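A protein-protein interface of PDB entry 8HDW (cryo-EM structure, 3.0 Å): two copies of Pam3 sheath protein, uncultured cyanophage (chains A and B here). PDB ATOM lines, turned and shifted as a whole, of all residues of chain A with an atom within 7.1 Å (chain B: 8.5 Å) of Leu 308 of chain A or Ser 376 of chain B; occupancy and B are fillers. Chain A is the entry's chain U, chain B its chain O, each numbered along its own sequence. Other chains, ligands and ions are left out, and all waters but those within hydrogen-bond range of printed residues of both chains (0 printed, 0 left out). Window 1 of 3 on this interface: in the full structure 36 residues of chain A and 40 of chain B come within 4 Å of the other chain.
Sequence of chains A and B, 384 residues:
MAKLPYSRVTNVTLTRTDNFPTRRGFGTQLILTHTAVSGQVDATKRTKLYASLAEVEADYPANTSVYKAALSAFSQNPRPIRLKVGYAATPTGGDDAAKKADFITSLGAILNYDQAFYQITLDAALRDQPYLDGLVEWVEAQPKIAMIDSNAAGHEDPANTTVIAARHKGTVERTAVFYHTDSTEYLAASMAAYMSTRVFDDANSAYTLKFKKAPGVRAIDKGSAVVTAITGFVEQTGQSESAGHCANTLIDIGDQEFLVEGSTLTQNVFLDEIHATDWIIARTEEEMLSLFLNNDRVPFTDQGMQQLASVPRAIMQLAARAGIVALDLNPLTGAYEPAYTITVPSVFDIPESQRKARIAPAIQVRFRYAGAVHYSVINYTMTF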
ATOM      1  N   GLU A 285     -10.549 -19.857   3.422  1.00  0.00           N
ATOM      2  CA  GLU A 285     -11.776 -19.157   3.792  1.00  0.00           C
ATOM      3  C   GLU A 285     -12.329 -19.665   5.115  1.00  0.00           C
ATOM      4  O   GLU A 285     -12.711 -18.875   5.989  1.00  0.00           O
ATOM      5  CB  GLU A 285     -12.830 -19.328   2.703  1.00  0.00           C
ATOM      6  CG  GLU A 285     -12.450 -18.804   1.347  1.00  0.00           C
ATOM      7  CD  GLU A 285     -12.745 -17.340   1.194  1.00  0.00           C
ATOM      8  OE1 GLU A 285     -12.600 -16.600   2.186  1.00  0.00           O
ATOM      9  OE2 GLU A 285     -13.132 -16.925   0.084  1.00  0.00           O
ATOM     10  N   MET A 288     -10.118 -18.604   8.050  1.00  0.00           N
ATOM     11  CA  MET A 288     -10.302 -17.187   8.345  1.00  0.00           C
ATOM     12  C   MET A 288     -11.595 -16.948   9.104  1.00  0.00           C
ATOM     13  O   MET A 288     -11.614 -16.199  10.086  1.00  0.00           O
ATOM     14  CB  MET A 288     -10.297 -16.360   7.062  1.00  0.00           C
ATOM     15  CG  MET A 288      -8.946 -16.214   6.401  1.00  0.00           C
ATOM     16  SD  MET A 288      -7.775 -15.273   7.385  1.00  0.00           S
ATOM     17  CE  MET A 288      -8.769 -13.846   7.769  1.00  0.00           C
ATOM     18  N   LEU A 291     -11.294 -17.961  12.613  1.00  0.00           N
ATOM     19  CA  LEU A 291     -10.542 -16.980  13.382  1.00  0.00           C
ATOM     20  C   LEU A 291     -11.370 -15.778  13.810  1.00  0.00           C
ATOM     21  O   LEU A 291     -11.134 -15.235  14.887  1.00  0.00           O
ATOM     22  CB  LEU A 291      -9.336 -16.482  12.577  1.00  0.00           C
ATOM     23  CG  LEU A 291      -8.368 -15.507  13.243  1.00  0.00           C
ATOM     24  CD1 LEU A 291      -7.411 -16.250  14.142  1.00  0.00           C
ATOM     25  CD2 LEU A 291      -7.609 -14.717  12.202  1.00  0.00           C
ATOM     26  N   PHE A 292     -12.329 -15.346  12.994  1.00  0.00           N
ATOM     27  CA  PHE A 292     -13.155 -14.200  13.351  1.00  0.00           C
ATOM     28  C   PHE A 292     -14.204 -14.538  14.400  1.00  0.00           C
ATOM     29  O   PHE A 292     -14.740 -13.624  15.031  1.00  0.00           O
ATOM     30  CB  PHE A 292     -13.845 -13.640  12.110  1.00  0.00           C
ATOM     31  CG  PHE A 292     -13.001 -12.689  11.317  1.00  0.00           C
ATOM     32  CD1 PHE A 292     -12.171 -11.784  11.947  1.00  0.00           C
ATOM     33  CD2 PHE A 292     -13.045 -12.699   9.935  1.00  0.00           C
ATOM     34  CE1 PHE A 292     -11.405 -10.908  11.216  1.00  0.00           C
ATOM     35  CE2 PHE A 292     -12.277 -11.828   9.198  1.00  0.00           C
ATOM     36  CZ  PHE A 292     -11.456 -10.933   9.838  1.00  0.00           C
ATOM     37  N   VAL A 298     -10.135  -8.611  16.131  1.00  0.00           N
ATOM     38  CA  VAL A 298      -8.835  -8.592  15.475  1.00  0.00           C
ATOM     39  C   VAL A 298      -8.461  -7.129  15.254  1.00  0.00           C
ATOM     40  O   VAL A 298      -9.077  -6.454  14.420  1.00  0.00           O
ATOM     41  CB  VAL A 298      -8.846  -9.377  14.156  1.00  0.00           C
ATOM     42  CG1 VAL A 298      -7.491  -9.305  13.486  1.00  0.00           C
ATOM     43  CG2 VAL A 298      -9.209 -10.817  14.416  1.00  0.00           C
ATOM     44  N   PRO A 299      -7.485  -6.592  15.980  1.00  0.00           N
ATOM     45  CA  PRO A 299      -7.194  -5.161  15.888  1.00  0.00           C
ATOM     46  C   PRO A 299      -6.530  -4.784  14.572  1.00  0.00           C
ATOM     47  O   PRO A 299      -5.950  -5.611  13.870  1.00  0.00           O
ATOM     48  CB  PRO A 299      -6.253  -4.923  17.070  1.00  0.00           C
ATOM     49  CG  PRO A 299      -5.592  -6.224  17.272  1.00  0.00           C
ATOM     50  CD  PRO A 299      -6.613  -7.269  16.949  1.00  0.00           C
ATOM     51  N   ASP A 302      -0.208  -3.977  13.491  1.00  0.00           N
ATOM     52  CA  ASP A 302       0.693  -4.981  12.931  1.00  0.00           C
ATOM     53  C   ASP A 302       0.510  -6.337  13.599  1.00  0.00           C
ATOM     54  O   ASP A 302       0.663  -7.380  12.949  1.00  0.00           O
ATOM     55  CB  ASP A 302       2.141  -4.522  13.062  1.00  0.00           C
ATOM     56  CG  ASP A 302       2.474  -3.366  12.138  1.00  0.00           C
ATOM     57  OD1 ASP A 302       1.819  -3.234  11.083  1.00  0.00           O
ATOM     58  OD2 ASP A 302       3.399  -2.594  12.463  1.00  0.00           O
ATOM     59  N   GLN A 303       0.190  -6.343  14.894  1.00  0.00           N
ATOM     60  CA  GLN A 303      -0.106  -7.591  15.588  1.00  0.00           C
ATOM     61  C   GLN A 303      -1.310  -8.284  14.970  1.00  0.00           C
ATOM     62  O   GLN A 303      -1.328  -9.511  14.819  1.00  0.00           O
ATOM     63  CB  GLN A 303      -0.342  -7.320  17.072  1.00  0.00           C
ATOM     64  CG  GLN A 303       0.922  -7.278  17.909  1.00  0.00           C
ATOM     65  CD  GLN A 303       1.767  -6.056  17.639  1.00  0.00           C
ATOM     66  OE1 GLN A 303       1.345  -5.135  16.943  1.00  0.00           O
ATOM     67  NE2 GLN A 303       2.967  -6.037  18.197  1.00  0.00           N
ATOM     68  N   GLY A 304      -2.332  -7.510  14.604  1.00  0.00           N
ATOM     69  CA  GLY A 304      -3.461  -8.066  13.887  1.00  0.00           C
ATOM     70  C   GLY A 304      -3.114  -8.617  12.524  1.00  0.00           C
ATOM     71  O   GLY A 304      -3.647  -9.659  12.138  1.00  0.00           O
ATOM     72  N   MET A 305      -2.231  -7.943  11.786  1.00  0.00           N
ATOM     73  CA  MET A 305      -1.801  -8.455  10.488  1.00  0.00           C
ATOM     74  C   MET A 305      -1.077  -9.785  10.631  1.00  0.00           C
ATOM     75  O   MET A 305      -1.278 -10.699   9.827  1.00  0.00           O
ATOM     76  CB  MET A 305      -0.908  -7.437   9.783  1.00  0.00           C
ATOM     77  CG  MET A 305      -1.549  -6.091   9.562  1.00  0.00           C
ATOM     78  SD  MET A 305      -3.189  -6.190   8.811  1.00  0.00           S
ATOM     79  CE  MET A 305      -2.822  -6.992   7.251  1.00  0.00           C
ATOM     80  N   GLN A 306      -0.216  -9.913  11.640  1.00  0.00           N
ATOM     81  CA  GLN A 306       0.442 -11.198  11.858  1.00  0.00           C
ATOM     82  C   GLN A 306      -0.546 -12.272  12.302  1.00  0.00           C
ATOM     83  O   GLN A 306      -0.440 -13.431  11.878  1.00  0.00           O
ATOM     84  CB  GLN A 306       1.567 -11.045  12.875  1.00  0.00           C
ATOM     85  CG  GLN A 306       2.758 -10.268  12.354  1.00  0.00           C
ATOM     86  CD  GLN A 306       3.527 -11.014  11.287  1.00  0.00           C
ATOM     87  OE1 GLN A 306       3.314 -12.201  11.066  1.00  0.00           O
ATOM     88  NE2 GLN A 306       4.434 -10.319  10.621  1.00  0.00           N
ATOM     89  N   GLN A 307      -1.524 -11.910  13.133  1.00  0.00           N
ATOM     90  CA  GLN A 307      -2.554 -12.869  13.514  1.00  0.00           C
ATOM     91  C   GLN A 307      -3.336 -13.352  12.297  1.00  0.00           C
ATOM     92  O   GLN A 307      -3.657 -14.540  12.190  1.00  0.00           O
ATOM     93  CB  GLN A 307      -3.488 -12.241  14.547  1.00  0.00           C
ATOM     94  CG  GLN A 307      -4.453 -13.215  15.183  1.00  0.00           C
ATOM     95  CD  GLN A 307      -5.278 -12.596  16.292  1.00  0.00           C
ATOM     96  OE1 GLN A 307      -5.168 -11.409  16.580  1.00  0.00           O
ATOM     97  NE2 GLN A 307      -6.108 -13.406  16.922  1.00  0.00           N
ATOM     98  N   LEU A 308      -3.660 -12.445  11.374  1.00  0.00           N
ATOM     99  CA  LEU A 308      -4.336 -12.847  10.143  1.00  0.00           C
ATOM    100  C   LEU A 308      -3.445 -13.727   9.278  1.00  0.00           C
ATOM    101  O   LEU A 308      -3.901 -14.738   8.739  1.00  0.00           O
ATOM    102  CB  LEU A 308      -4.779 -11.618   9.349  1.00  0.00           C
ATOM    103  CG  LEU A 308      -5.900 -10.738   9.892  1.00  0.00           C
ATOM    104  CD1 LEU A 308      -6.147  -9.583   8.956  1.00  0.00           C
ATOM    105  CD2 LEU A 308      -7.168 -11.538  10.085  1.00  0.00           C
ATOM    106  N   ALA A 309      -2.173 -13.358   9.130  1.00  0.00           N
ATOM    107  CA  ALA A 309      -1.272 -14.097   8.255  1.00  0.00           C
ATOM    108  C   ALA A 309      -0.891 -15.453   8.821  1.00  0.00           C
ATOM    109  O   ALA A 309      -0.295 -16.261   8.104  1.00  0.00           O
ATOM    110  CB  ALA A 309      -0.014 -13.280   7.989  1.00  0.00           C
ATOM    111  N   SER A 310      -1.194 -15.712  10.093  1.00  0.00           N
ATOM    112  CA  SER A 310      -0.941 -17.039  10.645  1.00  0.00           C
ATOM    113  C   SER A 310      -1.750 -18.137   9.963  1.00  0.00           C
ATOM    114  O   SER A 310      -1.401 -19.313  10.104  1.00  0.00           O
ATOM    115  CB  SER A 310      -1.231 -17.049  12.145  1.00  0.00           C
ATOM    116  OG  SER A 310      -2.601 -16.813  12.409  1.00  0.00           O
ATOM    117  N   VAL A 311      -2.812 -17.793   9.239  1.00  0.00           N
ATOM    118  CA  VAL A 311      -3.712 -18.776   8.634  1.00  0.00           C
ATOM    119  C   VAL A 311      -3.117 -19.371   7.357  1.00  0.00           C
ATOM    120  O   VAL A 311      -3.031 -20.609   7.250  1.00  0.00           O
ATOM    121  CB  VAL A 311      -5.103 -18.160   8.386  1.00  0.00           C
ATOM    122  CG1 VAL A 311      -5.903 -18.994   7.405  1.00  0.00           C
ATOM    123  CG2 VAL A 311      -5.855 -18.021   9.688  1.00  0.00           C
ATOM    124  N   PRO A 312      -2.695 -18.572   6.366  1.00  0.00           N
ATOM    125  CA  PRO A 312      -2.039 -19.179   5.199  1.00  0.00           C
ATOM    126  C   PRO A 312      -0.787 -19.963   5.538  1.00  0.00           C
ATOM    127  O   PRO A 312      -0.466 -20.917   4.825  1.00  0.00           O
ATOM    128  CB  PRO A 312      -1.725 -17.976   4.299  1.00  0.00           C
ATOM    129  CG  PRO A 312      -1.842 -16.807   5.154  1.00  0.00           C
ATOM    130  CD  PRO A 312      -2.878 -17.127   6.160  1.00  0.00           C
ATOM    131  N   ARG A 313      -0.073 -19.606   6.605  1.00  0.00           N
ATOM    132  CA  ARG A 313       1.104 -20.375   6.988  1.00  0.00           C
ATOM    133  C   ARG A 313       0.764 -21.805   7.365  1.00  0.00           C
ATOM    134  O   ARG A 313       1.501 -22.719   6.992  1.00  0.00           O
ATOM    135  CB  ARG A 313       1.829 -19.712   8.152  1.00  0.00           C
ATOM    136  CG  ARG A 313       2.598 -18.476   7.775  1.00  0.00           C
ATOM    137  CD  ARG A 313       3.546 -18.058   8.873  1.00  0.00           C
ATOM    138  NE  ARG A 313       4.143 -16.766   8.573  1.00  0.00           N
ATOM    139  CZ  ARG A 313       3.830 -15.635   9.193  1.00  0.00           C
ATOM    140  NH1 ARG A 313       2.936 -15.631  10.169  1.00  0.00           N
ATOM    141  NH2 ARG A 313       4.424 -14.507   8.839  1.00  0.00           N
ATOM    142  N   VAL A 344       3.738 -10.270   4.641  1.00  0.00           N
ATOM    143  CA  VAL A 344       2.697  -9.551   5.361  1.00  0.00           C
ATOM    144  C   VAL A 344       2.917  -8.058   5.155  1.00  0.00           C
ATOM    145  O   VAL A 344       4.036  -7.571   5.330  1.00  0.00           O
ATOM    146  CB  VAL A 344       2.708  -9.898   6.858  1.00  0.00           C
ATOM    147  CG1 VAL A 344       1.451  -9.403   7.542  1.00  0.00           C
ATOM    148  CG2 VAL A 344       2.873 -11.388   7.044  1.00  0.00           C
ATOM    149  N   ARG A 358     -11.875  -0.299   7.721  1.00  0.00           N
ATOM    150  CA  ARG A 358     -12.068  -1.618   8.327  1.00  0.00           C
ATOM    151  C   ARG A 358     -11.879  -2.731   7.303  1.00  0.00           C
ATOM    152  O   ARG A 358     -12.358  -3.850   7.479  1.00  0.00           O
ATOM    153  CB  ARG A 358     -13.423  -1.729   9.024  1.00  0.00           C
ATOM    154  CG  ARG A 358     -13.577  -0.760  10.172  1.00  0.00           C
ATOM    155  CD  ARG A 358     -14.243  -1.400  11.371  1.00  0.00           C
ATOM    156  NE  ARG A 358     -14.273  -0.488  12.508  1.00  0.00           N
ATOM    157  CZ  ARG A 358     -14.755  -0.798  13.706  1.00  0.00           C
ATOM    158  NH1 ARG A 358     -15.254  -2.004  13.928  1.00  0.00           N
ATOM    159  NH2 ARG A 358     -14.738   0.096  14.683  1.00  0.00           N
ATOM    160  N   ILE A 359     -11.156  -2.422   6.232  1.00  0.00           N
ATOM    161  CA  ILE A 359     -10.758  -3.403   5.233  1.00  0.00           C
ATOM    162  C   ILE A 359      -9.249  -3.538   5.307  1.00  0.00           C
ATOM    163  O   ILE A 359      -8.525  -2.577   5.026  1.00  0.00           O
ATOM    164  CB  ILE A 359     -11.194  -3.000   3.818  1.00  0.00           C
ATOM    165  CG1 ILE A 359     -12.712  -2.935   3.735  1.00  0.00           C
ATOM    166  CG2 ILE A 359     -10.654  -3.979   2.807  1.00  0.00           C
ATOM    167  CD1 ILE A 359     -13.212  -1.609   3.293  1.00  0.00           C
ATOM    168  N   ALA A 360      -8.779  -4.716   5.680  1.00  0.00           N
ATOM    169  CA  ALA A 360      -7.362  -4.941   5.876  1.00  0.00           C
ATOM    170  C   ALA A 360      -6.614  -4.941   4.548  1.00  0.00           C
ATOM    171  O   ALA A 360      -7.182  -5.261   3.502  1.00  0.00           O
ATOM    172  CB  ALA A 360      -7.141  -6.264   6.598  1.00  0.00           C
ATOM    173  N   PRO A 361      -5.332  -4.576   4.562  1.00  0.00           N
ATOM    174  CA  PRO A 361      -4.515  -4.715   3.350  1.00  0.00           C
ATOM    175  C   PRO A 361      -4.291  -6.165   2.956  1.00  0.00           C
ATOM    176  O   PRO A 361      -4.505  -7.077   3.760  1.00  0.00           O
ATOM    177  CB  PRO A 361      -3.202  -4.029   3.735  1.00  0.00           C
ATOM    178  CG  PRO A 361      -3.189  -4.031   5.217  1.00  0.00           C
ATOM    179  CD  PRO A 361      -4.604  -3.885   5.636  1.00  0.00           C
ATOM    180  N   ALA A 362      -3.846  -6.388   1.724  1.00  0.00           N
ATOM    181  CA  ALA A 362      -3.764  -7.719   1.142  1.00  0.00           C
ATOM    182  C   ALA A 362      -2.474  -8.424   1.538  1.00  0.00           C
ATOM    183  O   ALA A 362      -1.404  -7.814   1.574  1.00  0.00           O
ATOM    184  CB  ALA A 362      -3.859  -7.646  -0.380  1.00  0.00           C
ATOM    185  N   ILE A 363      -2.587  -9.711   1.821  1.00  0.00           N
ATOM    186  CA  ILE A 363      -1.450 -10.578   2.103  1.00  0.00           C
ATOM    187  C   ILE A 363      -1.150 -11.401   0.858  1.00  0.00           C
ATOM    188  O   ILE A 363      -2.062 -11.937   0.223  1.00  0.00           O
ATOM    189  CB  ILE A 363      -1.744 -11.479   3.315  1.00  0.00           C
ATOM    190  CG1 ILE A 363      -1.992 -10.625   4.555  1.00  0.00           C
ATOM    191  CG2 ILE A 363      -0.603 -12.439   3.560  1.00  0.00           C
ATOM    192  CD1 ILE A 363      -2.684 -11.356   5.672  1.00  0.00           C
ATOM    193  N   PHE B 211     -19.232  -7.749  15.317  1.00  0.00           N
ATOM    194  CA  PHE B 211     -19.490  -8.013  13.910  1.00  0.00           C
ATOM    195  C   PHE B 211     -19.624  -9.489  13.580  1.00  0.00           C
ATOM    196  O   PHE B 211     -20.250  -9.817  12.571  1.00  0.00           O
ATOM    197  CB  PHE B 211     -18.373  -7.384  13.064  1.00  0.00           C
ATOM    198  CG  PHE B 211     -18.447  -7.682  11.588  1.00  0.00           C
ATOM    199  CD1 PHE B 211     -19.617  -7.566  10.887  1.00  0.00           C
ATOM    200  CD2 PHE B 211     -17.307  -8.019  10.894  1.00  0.00           C
ATOM    201  CE1 PHE B 211     -19.655  -7.833   9.534  1.00  0.00           C
ATOM    202  CE2 PHE B 211     -17.350  -8.282   9.546  1.00  0.00           C
ATOM    203  CZ  PHE B 211     -18.524  -8.183   8.867  1.00  0.00           C
ATOM    204  N   PHE B 233     -23.612  -3.169   2.429  1.00  0.00           N
ATOM    205  CA  PHE B 233     -22.202  -3.532   2.471  1.00  0.00           C
ATOM    206  C   PHE B 233     -21.761  -4.047   1.107  1.00  0.00           C
ATOM    207  O   PHE B 233     -22.286  -5.055   0.622  1.00  0.00           O
ATOM    208  CB  PHE B 233     -21.948  -4.583   3.550  1.00  0.00           C
ATOM    209  CG  PHE B 233     -20.508  -4.995   3.672  1.00  0.00           C
ATOM    210  CD1 PHE B 233     -19.615  -4.235   4.405  1.00  0.00           C
ATOM    211  CD2 PHE B 233     -20.047  -6.152   3.066  1.00  0.00           C
ATOM    212  CE1 PHE B 233     -18.288  -4.615   4.519  1.00  0.00           C
ATOM    213  CE2 PHE B 233     -18.722  -6.535   3.184  1.00  0.00           C
ATOM    214  CZ  PHE B 233     -17.845  -5.764   3.908  1.00  0.00           C
ATOM    215  N   GLU B 235     -18.520  -5.524  -1.305  1.00  0.00           N
ATOM    216  CA  GLU B 235     -17.620  -6.628  -0.982  1.00  0.00           C
ATOM    217  C   GLU B 235     -16.327  -6.139  -0.341  1.00  0.00           C
ATOM    218  O   GLU B 235     -16.077  -6.389   0.842  1.00  0.00           O
ATOM    219  CB  GLU B 235     -17.315  -7.426  -2.248  1.00  0.00           C
ATOM    220  CG  GLU B 235     -17.067  -8.903  -2.019  1.00  0.00           C
ATOM    221  CD  GLU B 235     -18.331  -9.668  -1.674  1.00  0.00           C
ATOM    222  OE1 GLU B 235     -18.901  -9.430  -0.588  1.00  0.00           O
ATOM    223  OE2 GLU B 235     -18.758 -10.506  -2.496  1.00  0.00           O
ATOM    224  N   GLN B 236     -15.502  -5.429  -1.100  1.00  0.00           N
ATOM    225  CA  GLN B 236     -14.177  -5.036  -0.640  1.00  0.00           C
ATOM    226  C   GLN B 236     -14.036  -3.532  -0.486  1.00  0.00           C
ATOM    227  O   GLN B 236     -13.134  -3.066   0.218  1.00  0.00           O
ATOM    228  CB  GLN B 236     -13.124  -5.579  -1.617  1.00  0.00           C
ATOM    229  CG  GLN B 236     -11.702  -5.575  -1.109  1.00  0.00           C
ATOM    230  CD  GLN B 236     -10.765  -6.306  -2.046  1.00  0.00           C
ATOM    231  OE1 GLN B 236     -11.203  -6.998  -2.963  1.00  0.00           O
ATOM    232  NE2 GLN B 236      -9.467  -6.155  -1.822  1.00  0.00           N
ATOM    233  N   ALA B 372     -10.516  -1.824  14.416  1.00  0.00           N
ATOM    234  CA  ALA B 372     -10.203  -3.230  14.213  1.00  0.00           C
ATOM    235  C   ALA B 372     -10.560  -3.610  12.778  1.00  0.00           C
ATOM    236  O   ALA B 372     -10.900  -2.753  11.960  1.00  0.00           O
ATOM    237  CB  ALA B 372     -10.911  -4.084  15.268  1.00  0.00           C
ATOM    238  N   VAL B 373     -10.484  -4.905  12.473  1.00  0.00           N
ATOM    239  CA  VAL B 373     -10.510  -5.410  11.102  1.00  0.00           C
ATOM    240  C   VAL B 373     -11.828  -6.128  10.846  1.00  0.00           C
ATOM    241  O   VAL B 373     -12.272  -6.931  11.672  1.00  0.00           O
ATOM    242  CB  VAL B 373      -9.325  -6.355  10.827  1.00  0.00           C
ATOM    243  CG1 VAL B 373      -9.452  -6.983   9.462  1.00  0.00           C
ATOM    244  CG2 VAL B 373      -8.020  -5.610  10.939  1.00  0.00           C
ATOM    245  N   HIS B 374     -12.447  -5.843   9.695  1.00  0.00           N
ATOM    246  CA  HIS B 374     -13.671  -6.506   9.268  1.00  0.00           C
ATOM    247  C   HIS B 374     -13.512  -7.389   8.040  1.00  0.00           C
ATOM    248  O   HIS B 374     -14.381  -8.230   7.796  1.00  0.00           O
ATOM    249  CB  HIS B 374     -14.765  -5.473   8.961  1.00  0.00           C
ATOM    250  CG  HIS B 374     -15.527  -5.022  10.163  1.00  0.00           C
ATOM    251  ND1 HIS B 374     -16.712  -4.324  10.075  1.00  0.00           N
ATOM    252  CD2 HIS B 374     -15.276  -5.170  11.482  1.00  0.00           C
ATOM    253  CE1 HIS B 374     -17.157  -4.064  11.290  1.00  0.00           C
ATOM    254  NE2 HIS B 374     -16.302  -4.567  12.163  1.00  0.00           N
ATOM    255  N   TYR B 375     -12.445  -7.224   7.263  1.00  0.00           N
ATOM    256  CA  TYR B 375     -12.341  -7.833   5.948  1.00  0.00           C
ATOM    257  C   TYR B 375     -10.870  -8.068   5.643  1.00  0.00           C
ATOM    258  O   TYR B 375     -10.027  -7.223   5.942  1.00  0.00           O
ATOM    259  CB  TYR B 375     -12.993  -6.929   4.895  1.00  0.00           C
ATOM    260  CG  TYR B 375     -13.390  -7.612   3.613  1.00  0.00           C
ATOM    261  CD1 TYR B 375     -14.601  -8.266   3.502  1.00  0.00           C
ATOM    262  CD2 TYR B 375     -12.560  -7.584   2.505  1.00  0.00           C
ATOM    263  CE1 TYR B 375     -14.970  -8.887   2.333  1.00  0.00           C
ATOM    264  CE2 TYR B 375     -12.918  -8.201   1.337  1.00  0.00           C
ATOM    265  CZ  TYR B 375     -14.125  -8.852   1.253  1.00  0.00           C
ATOM    266  OH  TYR B 375     -14.487  -9.468   0.081  1.00  0.00           O
ATOM    267  N   SER B 376     -10.568  -9.219   5.043  1.00  0.00           N
ATOM    268  CA  SER B 376      -9.193  -9.637   4.803  1.00  0.00           C
ATOM    269  C   SER B 376      -9.000  -9.967   3.332  1.00  0.00           C
ATOM    270  O   SER B 376      -9.956 -10.292   2.626  1.00  0.00           O
ATOM    271  CB  SER B 376      -8.824 -10.858   5.643  1.00  0.00           C
ATOM    272  OG  SER B 376      -9.202 -10.675   6.988  1.00  0.00           O
ATOM    273  N   VAL B 377      -7.751  -9.882   2.874  1.00  0.00           N
ATOM    274  CA  VAL B 377      -7.392 -10.146   1.482  1.00  0.00           C
ATOM    275  C   VAL B 377      -6.118 -10.981   1.447  1.00  0.00           C
ATOM    276  O   VAL B 377      -5.173 -10.706   2.192  1.00  0.00           O
ATOM    277  CB  VAL B 377      -7.196  -8.843   0.684  1.00  0.00           C
ATOM    278  CG1 VAL B 377      -7.074  -9.149  -0.791  1.00  0.00           C
ATOM    279  CG2 VAL B 377      -8.333  -7.869   0.937  1.00  0.00           C
ATOM    280  N   ILE B 378      -6.093 -12.004   0.588  1.00  0.00           N
ATOM    281  CA  ILE B 378      -4.923 -12.845   0.352  1.00  0.00           C
ATOM    282  C   ILE B 378      -4.818 -13.109  -1.145  1.00  0.00           C
ATOM    283  O   ILE B 378      -5.825 -13.357  -1.813  1.00  0.00           O
ATOM    284  CB  ILE B 378      -4.995 -14.173   1.138  1.00  0.00           C
ATOM    285  CG1 ILE B 378      -4.989 -13.914   2.640  1.00  0.00           C
ATOM    286  CG2 ILE B 378      -3.843 -15.081   0.768  1.00  0.00           C
ATOM    287  CD1 ILE B 378      -4.860 -15.161   3.465  1.00  0.00           C
ATOM    288  N   ASN B 379      -3.593 -13.072  -1.676  1.00  0.00           N
ATOM    289  CA  ASN B 379      -3.398 -13.034  -3.126  1.00  0.00           C
ATOM    290  C   ASN B 379      -3.020 -14.362  -3.773  1.00  0.00           C
ATOM    291  O   ASN B 379      -3.623 -14.715  -4.787  1.00  0.00           O
ATOM    292  CB  ASN B 379      -2.355 -11.979  -3.485  1.00  0.00           C
ATOM    293  CG  ASN B 379      -2.916 -10.579  -3.421  1.00  0.00           C
ATOM    294  OD1 ASN B 379      -4.128 -10.389  -3.419  1.00  0.00           O
ATOM    295  ND2 ASN B 379      -2.036  -9.589  -3.372  1.00  0.00           N
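The backbone NH (N) of Tyr 375 of chain B is in hydrogen-bond range of the backbone carbonyl oxygen (O) of Arg 358 of chain A (3.4 Å).
N of Ile 363 of chain A lies within hydrogen-bond range of O of Val 377 of chain B, 2.8 Å away.
The backbone NH of Asn 379 of chain B lies within hydrogen-bond range of the backbone carbonyl oxygen of Ile 363 of chain A, 2.7 Å away.
The backbone carbonyl oxygen (O) of Tyr 375 of chain B lies within hydrogen-bond range of the backbone NH (N) of Ala 360 of chain A (2.8 Å).
The backbone carbonyl oxygen of Val 298 of chain A sits at hydrogen-bond distance from the backbone NH of Val 373 of chain B (2.9 Å).
The backbone carbonyl oxygen of Arg 358 of chain A is in hydrogen-bond range of the backbone NH of His 374 of chain B (3.0 Å).
No position is printed for both chains.
Of the 20 pairs that touch across the chains among the printed residues, none has its exchanged pair printed and touching as well.
Printed residues of chain B within 4 Å of Pro 299 of chain A: Ala 372 (3.9 Å) and Val 373 (3.6 Å).
Leu 308 of chain A touches just one residue of chain B: Ser 376 (3.8 Å).
No residue of chain B comes within 4 Å of Ala 309 of chain A.
Arg 313 of chain A touches none of the printed residues of chain B.
Of the printed residues of chain A, Tyr 375 of chain B touches Arg 358 (3.4 Å), Ile 359 (3.8 Å) and Ala 360 (2.8 Å).
Of chain A, only Met 288, Phe 292 and Leu 308 come within 4 Å of Ser 376 of chain B.
The nearest residue of chain B that does not touch Leu 308 of chain A is Val 373 of chain B (4.2 Å).
The nearest residue of chain A that does not touch Ser 376 of chain B is Ala 360 of chain A (4.3 Å).
Of the 12 printed residues of chain B, 9 touch a printed residue of chain A.
Of the 25 printed residues of chain A, 11 touch a printed residue of chain B.
Printed residues of chain A that touch a printed residue of chain B: Met 288, Phe 292, Val 298, Pro 299, Leu 308, Pro 312, Arg 358, Ile 359, Ala 360, Ala 362 and Ile 363.
Hydrophobic or aromatic side chains of chain A that line the printed part of chain B: Met 288, Phe 292, Leu 308, Pro 312, Ile 359, Ala 360, Ala 362 and Ile 363.
Among the printed residues, 20 pairs touch across the chains.
Among the printed residues, no Asp or Glu carboxylate lies within 4 Å of a Lys or Arg side-chain nitrogen of the other chain.
Among the printed residues, merely in contact across the chains: Ile 363 of chain A with Ile 378 of chain B (3.0 Å), Val 298 of chain A with Ala 372 of chain B (3.1 Å), Met 288 of chain A with Ser 376 of chain B (3.3 Å), Ile 359 of chain A with Gln 236 of chain B (3.4 Å), Ala 362 of chain A with Val 377 of chain B (3.5 Å), Pro 299 of chain A with Val 373 of chain B (3.6 Å), Phe 292 of chain A with Ser 376 of chain B (3.6 Å), Arg 358 of chain A with Ala 372 of chain B (3.7 Å), Ala 360 of chain A with Val 373 of chain B (3.7 Å), Leu 308 of chain A with Ser 376 of chain B (3.8 Å), Ile 359 of chain A with Tyr 375 of chain B (3.8 Å), Pro 312 of chain A with Ile 378 of chain B (3.8 Å), Ala 360 of chain A with Val 377 of chain B (3.8 Å) and Pro 299 of chain A with Ala 372 of chain B (3.9 Å).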
